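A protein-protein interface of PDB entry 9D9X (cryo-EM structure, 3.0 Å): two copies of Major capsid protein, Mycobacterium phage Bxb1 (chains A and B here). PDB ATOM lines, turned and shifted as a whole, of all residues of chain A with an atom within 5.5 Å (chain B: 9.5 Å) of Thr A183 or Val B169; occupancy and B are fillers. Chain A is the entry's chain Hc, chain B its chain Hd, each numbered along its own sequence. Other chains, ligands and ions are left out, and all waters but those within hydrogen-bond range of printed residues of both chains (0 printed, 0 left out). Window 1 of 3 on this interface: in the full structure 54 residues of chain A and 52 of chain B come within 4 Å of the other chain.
The side-chain carboxylate (OE2) of Glu A185 is in salt-bridge range of the guanidinium group (NH2) of Arg B220, at 2.8 Å.
The side-chain carboxylate (OD1) of Asp A181 lies within hydrogen-bond range of the side-chain hydroxyl (OG1) of Thr A183 (2.6 Å). N of Leu B165 lies within hydrogen-bond range of O of Leu B160 (3.1 Å). O of Val B162 is in hydrogen-bond range of OG1 of Thr B166 (2.7 Å). O of Thr B166 is in hydrogen-bond range of OG1 of Thr B170 (2.7 Å). The guanidinium group of Arg B220 lies within hydrogen-bond range of the backbone carbonyl oxygen of Trp B175, 3.0 Å away.
Among the printed residues, pairs that only touch across the chains: Pro A186 with Thr B166 (3.4 Å), Glu A185 with Leu B165 (3.6 Å), Pro A186 with Val B162 (3.8 Å), Thr A183 with Val B169 (3.8 Å) and Pro A186 with Val B169 (3.9 Å).
Thr A183 touches just one residue of chain B: Val B169. Of chain A, only Thr A183 and Pro A186 come within 4 Å of Val B169. Of the printed residues of chain A, Val B162 touches Pro A186. Of the printed residues of chain B, Pro A186 touches Val B162 (3.8 Å), Thr B166 (3.4 Å) and Val B169 (3.9 Å). Asn B296 touches none of the printed residues of chain A. The nearest residue of chain A that does not touch Val B169 is Asp A182 (4.9 Å).
Of the 10 printed residues of chain A, 3 touch a printed residue of chain B. Printed residues of chain A that touch a printed residue of chain B: Thr A183, Glu A185 and Pro A186. Hydrophobic or aromatic side chains of chain A that line the printed part of chain B: Pro A186. Hydrophobic or aromatic side chains of chain B within 4 Å of the printed part of chain A: Val B162, Leu B165 and Val B169.
No position is printed for both chains. Of the 6 pairs that touch across the chains among the printed residues, none has its exchanged pair printed and touching as well.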
ATOM      1  N   ASP A 181      28.396  10.247  22.936  1.00  0.00           N
ATOM      2  CA  ASP A 181      27.622  11.432  23.284  1.00  0.00           C
ATOM      3  C   ASP A 181      26.914  12.053  22.069  1.00  0.00           C
ATOM      4  O   ASP A 181      27.469  12.069  20.978  1.00  0.00           O
ATOM      5  CB  ASP A 181      28.567  12.439  23.922  1.00  0.00           C
ATOM      6  CG  ASP A 181      27.782  13.549  24.604  1.00  0.00           C
ATOM      7  OD1 ASP A 181      27.483  14.549  23.909  1.00  0.00           O
ATOM      8  OD2 ASP A 181      27.517  13.416  25.819  1.00  0.00           O
ATOM      9  N   ASP A 182      25.733  12.646  22.229  1.00  0.00           N
ATOM     10  CA  ASP A 182      25.047  13.374  21.153  1.00  0.00           C
ATOM     11  C   ASP A 182      25.911  14.445  20.472  1.00  0.00           C
ATOM     12  O   ASP A 182      25.777  14.676  19.274  1.00  0.00           O
ATOM     13  CB  ASP A 182      23.788  14.058  21.698  1.00  0.00           C
ATOM     14  CG  ASP A 182      22.605  13.120  21.950  1.00  0.00           C
ATOM     15  OD1 ASP A 182      22.661  11.932  21.569  1.00  0.00           O
ATOM     16  OD2 ASP A 182      21.577  13.608  22.474  1.00  0.00           O
ATOM     17  N   THR A 183      26.831  15.088  21.183  1.00  0.00           N
ATOM     18  CA  THR A 183      27.744  16.081  20.596  1.00  0.00           C
ATOM     19  C   THR A 183      28.721  15.503  19.572  1.00  0.00           C
ATOM     20  O   THR A 183      29.418  16.259  18.903  1.00  0.00           O
ATOM     21  CB  THR A 183      28.534  16.810  21.676  1.00  0.00           C
ATOM     22  OG1 THR A 183      29.214  15.895  22.493  1.00  0.00           O
ATOM     23  CG2 THR A 183      27.636  17.651  22.571  1.00  0.00           C
ATOM     24  N   VAL A 184      28.766  14.186  19.388  1.00  0.00           N
ATOM     25  CA  VAL A 184      29.541  13.527  18.337  1.00  0.00           C
ATOM     26  C   VAL A 184      28.903  13.682  16.957  1.00  0.00           C
ATOM     27  O   VAL A 184      29.613  13.577  15.966  1.00  0.00           O
ATOM     28  CB  VAL A 184      29.764  12.046  18.697  1.00  0.00           C
ATOM     29  CG1 VAL A 184      30.542  11.258  17.643  1.00  0.00           C
ATOM     30  CG2 VAL A 184      30.572  11.935  19.992  1.00  0.00           C
ATOM     31  N   GLU A 185      27.603  13.980  16.837  1.00  0.00           N
ATOM     32  CA  GLU A 185      26.930  14.008  15.534  1.00  0.00           C
ATOM     33  C   GLU A 185      27.631  14.864  14.469  1.00  0.00           C
ATOM     34  O   GLU A 185      27.881  14.348  13.386  1.00  0.00           O
ATOM     35  CB  GLU A 185      25.454  14.407  15.655  1.00  0.00           C
ATOM     36  CG  GLU A 185      24.683  13.884  14.432  1.00  0.00           C
ATOM     37  CD  GLU A 185      23.326  14.560  14.183  1.00  0.00           C
ATOM     38  OE1 GLU A 185      22.583  14.860  15.143  1.00  0.00           O
ATOM     39  OE2 GLU A 185      22.963  14.772  13.003  1.00  0.00           O
ATOM     40  N   PRO A 186      28.031  16.120  14.711  1.00  0.00           N
ATOM     41  CA  PRO A 186      28.653  16.916  13.668  1.00  0.00           C
ATOM     42  C   PRO A 186      29.982  16.350  13.168  1.00  0.00           C
ATOM     43  O   PRO A 186      30.231  16.402  11.967  1.00  0.00           O
ATOM     44  CB  PRO A 186      28.812  18.318  14.245  1.00  0.00           C
ATOM     45  CG  PRO A 186      28.740  18.107  15.747  1.00  0.00           C
ATOM     46  CD  PRO A 186      27.782  16.939  15.876  1.00  0.00           C
ATOM     47  N   VAL A 187      30.827  15.765  14.025  1.00  0.00           N
ATOM     48  CA  VAL A 187      32.079  15.145  13.556  1.00  0.00           C
ATOM     49  C   VAL A 187      31.831  13.839  12.828  1.00  0.00           C
ATOM     50  O   VAL A 187      32.662  13.408  12.037  1.00  0.00           O
ATOM     51  CB  VAL A 187      33.134  14.925  14.647  1.00  0.00           C
ATOM     52  CG1 VAL A 187      33.423  16.217  15.414  1.00  0.00           C
ATOM     53  CG2 VAL A 187      32.817  13.818  15.648  1.00  0.00           C
ATOM     54  N   ALA A 229      29.641  12.790  27.688  1.00  0.00           N
ATOM     55  CA  ALA A 229      30.826  13.620  27.493  1.00  0.00           C
ATOM     56  C   ALA A 229      31.191  14.424  28.745  1.00  0.00           C
ATOM     57  O   ALA A 229      30.319  14.971  29.417  1.00  0.00           O
ATOM     58  CB  ALA A 229      30.618  14.557  26.301  1.00  0.00           C
ATOM     59  N   VAL A 234      34.370  12.139  24.713  1.00  0.00           N
ATOM     60  CA  VAL A 234      33.065  12.202  24.042  1.00  0.00           C
ATOM     61  C   VAL A 234      32.424  10.836  23.839  1.00  0.00           C
ATOM     62  O   VAL A 234      31.315  10.741  23.326  1.00  0.00           O
ATOM     63  CB  VAL A 234      33.161  12.954  22.712  1.00  0.00           C
ATOM     64  CG1 VAL A 234      33.610  14.396  22.931  1.00  0.00           C
ATOM     65  CG2 VAL A 234      34.120  12.292  21.725  1.00  0.00           C
ATOM     66  N   PHE A 303      38.170  14.503  20.713  1.00  0.00           N
ATOM     67  CA  PHE A 303      38.242  15.379  19.533  1.00  0.00           C
ATOM     68  C   PHE A 303      39.614  16.022  19.280  1.00  0.00           C
ATOM     69  O   PHE A 303      39.747  16.790  18.332  1.00  0.00           O
ATOM     70  CB  PHE A 303      37.205  16.503  19.662  1.00  0.00           C
ATOM     71  CG  PHE A 303      35.741  16.158  19.537  1.00  0.00           C
ATOM     72  CD1 PHE A 303      35.295  14.959  18.963  1.00  0.00           C
ATOM     73  CD2 PHE A 303      34.805  17.117  19.948  1.00  0.00           C
ATOM     74  CE1 PHE A 303      33.920  14.722  18.822  1.00  0.00           C
ATOM     75  CE2 PHE A 303      33.431  16.881  19.804  1.00  0.00           C
ATOM     76  CZ  PHE A 303      32.989  15.683  19.233  1.00  0.00           C
ATOM     77  N   LYS B 148      23.751  33.371  16.379  1.00  0.00           N
ATOM     78  CA  LYS B 148      24.328  32.325  15.519  1.00  0.00           C
ATOM     79  C   LYS B 148      24.023  32.548  14.041  1.00  0.00           C
ATOM     80  O   LYS B 148      22.855  32.591  13.657  1.00  0.00           O
ATOM     81  CB  LYS B 148      23.779  30.965  15.945  1.00  0.00           C
ATOM     82  CG  LYS B 148      24.203  30.569  17.355  1.00  0.00           C
ATOM     83  CD  LYS B 148      23.560  29.235  17.732  1.00  0.00           C
ATOM     84  CE  LYS B 148      24.023  28.771  19.110  1.00  0.00           C
ATOM     85  NZ  LYS B 148      23.472  29.617  20.191  1.00  0.00           N
ATOM     86  N   LEU B 160      24.934  23.151   6.677  1.00  0.00           N
ATOM     87  CA  LEU B 160      23.935  22.725   7.660  1.00  0.00           C
ATOM     88  C   LEU B 160      24.443  21.631   8.600  1.00  0.00           C
ATOM     89  O   LEU B 160      24.426  21.792   9.816  1.00  0.00           O
ATOM     90  CB  LEU B 160      22.677  22.223   6.941  1.00  0.00           C
ATOM     91  CG  LEU B 160      21.953  23.272   6.093  1.00  0.00           C
ATOM     92  CD1 LEU B 160      20.816  22.602   5.331  1.00  0.00           C
ATOM     93  CD2 LEU B 160      21.361  24.376   6.957  1.00  0.00           C
ATOM     94  N   GLY B 161      24.887  20.505   8.052  1.00  0.00           N
ATOM     95  CA  GLY B 161      25.066  19.259   8.791  1.00  0.00           C
ATOM     96  C   GLY B 161      26.357  19.144   9.588  1.00  0.00           C
ATOM     97  O   GLY B 161      26.497  18.204  10.364  1.00  0.00           O
ATOM     98  N   VAL B 162      27.299  20.072   9.422  1.00  0.00           N
ATOM     99  CA  VAL B 162      28.605  20.034  10.092  1.00  0.00           C
ATOM    100  C   VAL B 162      28.877  21.333  10.823  1.00  0.00           C
ATOM    101  O   VAL B 162      28.849  21.380  12.052  1.00  0.00           O
ATOM    102  CB  VAL B 162      29.735  19.691   9.113  1.00  0.00           C
ATOM    103  CG1 VAL B 162      31.084  19.592   9.819  1.00  0.00           C
ATOM    104  CG2 VAL B 162      29.474  18.365   8.412  1.00  0.00           C
ATOM    105  N   SER B 163      29.099  22.422  10.099  1.00  0.00           N
ATOM    106  CA  SER B 163      29.445  23.694  10.725  1.00  0.00           C
ATOM    107  C   SER B 163      28.252  24.327  11.439  1.00  0.00           C
ATOM    108  O   SER B 163      28.403  24.899  12.512  1.00  0.00           O
ATOM    109  CB  SER B 163      30.042  24.608   9.667  1.00  0.00           C
ATOM    110  OG  SER B 163      30.521  25.791  10.261  1.00  0.00           O
ATOM    111  N   GLY B 164      27.047  24.184  10.892  1.00  0.00           N
ATOM    112  CA  GLY B 164      25.818  24.707  11.475  1.00  0.00           C
ATOM    113  C   GLY B 164      25.430  23.955  12.734  1.00  0.00           C
ATOM    114  O   GLY B 164      25.328  24.550  13.797  1.00  0.00           O
ATOM    115  N   LEU B 165      25.296  22.635  12.651  1.00  0.00           N
ATOM    116  CA  LEU B 165      24.948  21.801  13.796  1.00  0.00           C
ATOM    117  C   LEU B 165      25.928  21.935  14.962  1.00  0.00           C
ATOM    118  O   LEU B 165      25.506  21.908  16.114  1.00  0.00           O
ATOM    119  CB  LEU B 165      24.847  20.353  13.315  1.00  0.00           C
ATOM    120  CG  LEU B 165      24.439  19.378  14.423  1.00  0.00           C
ATOM    121  CD1 LEU B 165      23.050  19.698  14.962  1.00  0.00           C
ATOM    122  CD2 LEU B 165      24.419  17.962  13.876  1.00  0.00           C
ATOM    123  N   THR B 166      27.216  22.152  14.699  1.00  0.00           N
ATOM    124  CA  THR B 166      28.214  22.376  15.752  1.00  0.00           C
ATOM    125  C   THR B 166      27.846  23.546  16.654  1.00  0.00           C
ATOM    126  O   THR B 166      27.945  23.426  17.874  1.00  0.00           O
ATOM    127  CB  THR B 166      29.603  22.604  15.159  1.00  0.00           C
ATOM    128  OG1 THR B 166      30.033  21.432  14.522  1.00  0.00           O
ATOM    129  CG2 THR B 166      30.659  22.913  16.214  1.00  0.00           C
ATOM    130  N   LYS B 167      27.357  24.657  16.095  1.00  0.00           N
ATOM    131  CA  LYS B 167      26.954  25.828  16.880  1.00  0.00           C
ATOM    132  C   LYS B 167      25.759  25.530  17.782  1.00  0.00           C
ATOM    133  O   LYS B 167      25.672  26.099  18.860  1.00  0.00           O
ATOM    134  CB  LYS B 167      26.634  27.001  15.945  1.00  0.00           C
ATOM    135  CG  LYS B 167      27.865  27.563  15.224  1.00  0.00           C
ATOM    136  CD  LYS B 167      27.438  28.695  14.276  1.00  0.00           C
ATOM    137  CE  LYS B 167      28.616  29.495  13.712  1.00  0.00           C
ATOM    138  NZ  LYS B 167      29.444  28.720  12.755  1.00  0.00           N
ATOM    139  N   LEU B 168      24.853  24.640  17.386  1.00  0.00           N
ATOM    140  CA  LEU B 168      23.700  24.262  18.202  1.00  0.00           C
ATOM    141  C   LEU B 168      24.066  23.285  19.316  1.00  0.00           C
ATOM    142  O   LEU B 168      23.740  23.545  20.469  1.00  0.00           O
ATOM    143  CB  LEU B 168      22.586  23.690  17.316  1.00  0.00           C
ATOM    144  CG  LEU B 168      21.884  24.747  16.455  1.00  0.00           C
ATOM    145  CD1 LEU B 168      20.962  24.064  15.457  1.00  0.00           C
ATOM    146  CD2 LEU B 168      21.016  25.691  17.282  1.00  0.00           C
ATOM    147  N   VAL B 169      24.751  22.182  19.017  1.00  0.00           N
ATOM    148  CA  VAL B 169      25.019  21.151  20.031  1.00  0.00           C
ATOM    149  C   VAL B 169      26.083  21.575  21.037  1.00  0.00           C
ATOM    150  O   VAL B 169      26.052  21.116  22.172  1.00  0.00           O
ATOM    151  CB  VAL B 169      25.344  19.777  19.433  1.00  0.00           C
ATOM    152  CG1 VAL B 169      24.203  19.289  18.546  1.00  0.00           C
ATOM    153  CG2 VAL B 169      26.649  19.736  18.643  1.00  0.00           C
ATOM    154  N   THR B 170      26.962  22.514  20.691  1.00  0.00           N
ATOM    155  CA  THR B 170      27.875  23.132  21.665  1.00  0.00           C
ATOM    156  C   THR B 170      27.125  23.869  22.778  1.00  0.00           C
ATOM    157  O   THR B 170      27.549  23.828  23.929  1.00  0.00           O
ATOM    158  CB  THR B 170      28.846  24.084  20.967  1.00  0.00           C
ATOM    159  OG1 THR B 170      29.596  23.366  20.021  1.00  0.00           O
ATOM    160  CG2 THR B 170      29.851  24.735  21.909  1.00  0.00           C
ATOM    161  N   ASP B 171      25.971  24.473  22.481  1.00  0.00           N
ATOM    162  CA  ASP B 171      25.077  25.086  23.472  1.00  0.00           C
ATOM    163  C   ASP B 171      23.968  24.142  23.968  1.00  0.00           C
ATOM    164  O   ASP B 171      23.054  24.570  24.667  1.00  0.00           O
ATOM    165  CB  ASP B 171      24.462  26.374  22.911  1.00  0.00           C
ATOM    166  CG  ASP B 171      25.436  27.537  22.724  1.00  0.00           C
ATOM    167  OD1 ASP B 171      26.625  27.434  23.092  1.00  0.00           O
ATOM    168  OD2 ASP B 171      24.973  28.595  22.238  1.00  0.00           O
ATOM    169  N   GLY B 172      23.996  22.860  23.619  1.00  0.00           N
ATOM    170  CA  GLY B 172      22.983  21.902  24.063  1.00  0.00           C
ATOM    171  C   GLY B 172      21.590  22.101  23.462  1.00  0.00           C
ATOM    172  O   GLY B 172      20.613  21.585  24.004  1.00  0.00           O
ATOM    173  N   LYS B 173      21.467  22.839  22.356  1.00  0.00           N
ATOM    174  CA  LYS B 173      20.221  22.963  21.580  1.00  0.00           C
ATOM    175  C   LYS B 173      20.060  21.769  20.630  1.00  0.00           C
ATOM    176  O   LYS B 173      21.039  21.099  20.316  1.00  0.00           O
ATOM    177  CB  LYS B 173      20.224  24.284  20.799  1.00  0.00           C
ATOM    178  CG  LYS B 173      20.711  25.518  21.575  1.00  0.00           C
ATOM    179  CD  LYS B 173      19.879  25.850  22.815  1.00  0.00           C
ATOM    180  CE  LYS B 173      20.611  26.937  23.603  1.00  0.00           C
ATOM    181  NZ  LYS B 173      19.870  27.350  24.817  1.00  0.00           N
ATOM    182  N   LYS B 174      18.854  21.524  20.117  1.00  0.00           N
ATOM    183  CA  LYS B 174      18.571  20.463  19.132  1.00  0.00           C
ATOM    184  C   LYS B 174      18.156  21.033  17.782  1.00  0.00           C
ATOM    185  O   LYS B 174      17.189  21.772  17.705  1.00  0.00           O
ATOM    186  CB  LYS B 174      17.481  19.526  19.665  1.00  0.00           C
ATOM    187  CG  LYS B 174      17.964  18.752  20.893  1.00  0.00           C
ATOM    188  CD  LYS B 174      16.917  17.775  21.433  1.00  0.00           C
ATOM    189  CE  LYS B 174      16.647  16.622  20.459  1.00  0.00           C
ATOM    190  NZ  LYS B 174      15.779  15.587  21.070  1.00  0.00           N
ATOM    191  N   TRP B 175      18.810  20.650  16.693  1.00  0.00           N
ATOM    192  CA  TRP B 175      18.316  20.930  15.344  1.00  0.00           C
ATOM    193  C   TRP B 175      17.148  20.006  15.007  1.00  0.00           C
ATOM    194  O   TRP B 175      17.373  18.817  14.789  1.00  0.00           O
ATOM    195  CB  TRP B 175      19.451  20.722  14.340  1.00  0.00           C
ATOM    196  CG  TRP B 175      19.089  20.905  12.903  1.00  0.00           C
ATOM    197  CD1 TRP B 175      18.155  21.751  12.430  1.00  0.00           C
ATOM    198  CD2 TRP B 175      19.690  20.286  11.728  1.00  0.00           C
ATOM    199  NE1 TRP B 175      18.120  21.680  11.060  1.00  0.00           N
ATOM    200  CE2 TRP B 175      19.044  20.796  10.570  1.00  0.00           C
ATOM    201  CE3 TRP B 175      20.708  19.338  11.518  1.00  0.00           C
ATOM    202  CZ2 TRP B 175      19.388  20.395   9.277  1.00  0.00           C
ATOM    203  CZ3 TRP B 175      21.068  18.930  10.224  1.00  0.00           C
ATOM    204  CH2 TRP B 175      20.414  19.458   9.104  1.00  0.00           C
ATOM    205  N   THR B 176      15.914  20.511  14.950  1.00  0.00           N
ATOM    206  CA  THR B 176      14.745  19.672  14.629  1.00  0.00           C
ATOM    207  C   THR B 176      14.103  19.982  13.285  1.00  0.00           C
ATOM    208  O   THR B 176      13.537  19.076  12.687  1.00  0.00           O
ATOM    209  CB  THR B 176      13.673  19.703  15.719  1.00  0.00           C
ATOM    210  OG1 THR B 176      12.956  20.916  15.705  1.00  0.00           O
ATOM    211  CG2 THR B 176      14.242  19.515  17.119  1.00  0.00           C
ATOM    212  N   ARG B 220      15.955  15.755   9.466  1.00  0.00           N
ATOM    213  CA  ARG B 220      15.175  16.938   9.870  1.00  0.00           C
ATOM    214  C   ARG B 220      14.305  17.436   8.715  1.00  0.00           C
ATOM    215  O   ARG B 220      14.852  17.652   7.639  1.00  0.00           O
ATOM    216  CB  ARG B 220      16.113  18.078  10.299  1.00  0.00           C
ATOM    217  CG  ARG B 220      16.786  17.888  11.661  1.00  0.00           C
ATOM    218  CD  ARG B 220      17.926  16.874  11.648  1.00  0.00           C
ATOM    219  NE  ARG B 220      18.650  16.884  12.920  1.00  0.00           N
ATOM    220  CZ  ARG B 220      19.779  16.254  13.169  1.00  0.00           C
ATOM    221  NH1 ARG B 220      20.365  16.391  14.314  1.00  0.00           N
ATOM    222  NH2 ARG B 220      20.347  15.472  12.307  1.00  0.00           N
ATOM    223  N   ASN B 296      18.198  31.992  20.976  1.00  0.00           N
ATOM    224  CA  ASN B 296      19.490  31.398  20.653  1.00  0.00           C
ATOM    225  C   ASN B 296      19.394  29.915  20.265  1.00  0.00           C
ATOM    226  O   ASN B 296      20.421  29.297  20.008  1.00  0.00           O
ATOM    227  CB  ASN B 296      20.452  31.626  21.817  1.00  0.00           C
ATOM    228  CG  ASN B 296      20.501  33.074  22.229  1.00  0.00           C
ATOM    229  OD1 ASN B 296      21.179  33.887  21.627  1.00  0.00           O
ATOM    230  ND2 ASN B 296      19.767  33.436  23.251  1.00  0.00           N
ATOM    231  N   ALA B 297      18.193  29.340  20.206  1.00  0.00           N
ATOM    232  CA  ALA B 297      17.944  27.985  19.725  1.00  0.00           C
ATOM    233  C   ALA B 297      17.888  27.857  18.191  1.00  0.00           C
ATOM    234  O   ALA B 297      17.566  26.788  17.678  1.00  0.00           O
ATOM    235  CB  ALA B 297      16.650  27.490  20.374  1.00  0.00           C
ATOM    236  N   VAL B 299      19.759  29.029  14.232  1.00  0.00           N
ATOM    237  CA  VAL B 299      20.858  29.527  13.411  1.00  0.00           C
ATOM    238  C   VAL B 299      20.272  30.246  12.213  1.00  0.00           C
ATOM    239  O   VAL B 299      19.426  29.698  11.519  1.00  0.00           O
ATOM    240  CB  VAL B 299      21.759  28.385  12.938  1.00  0.00           C
ATOM    241  CG1 VAL B 299      22.953  28.912  12.149  1.00  0.00           C
ATOM    242  CG2 VAL B 299      22.305  27.579  14.109  1.00  0.00           C
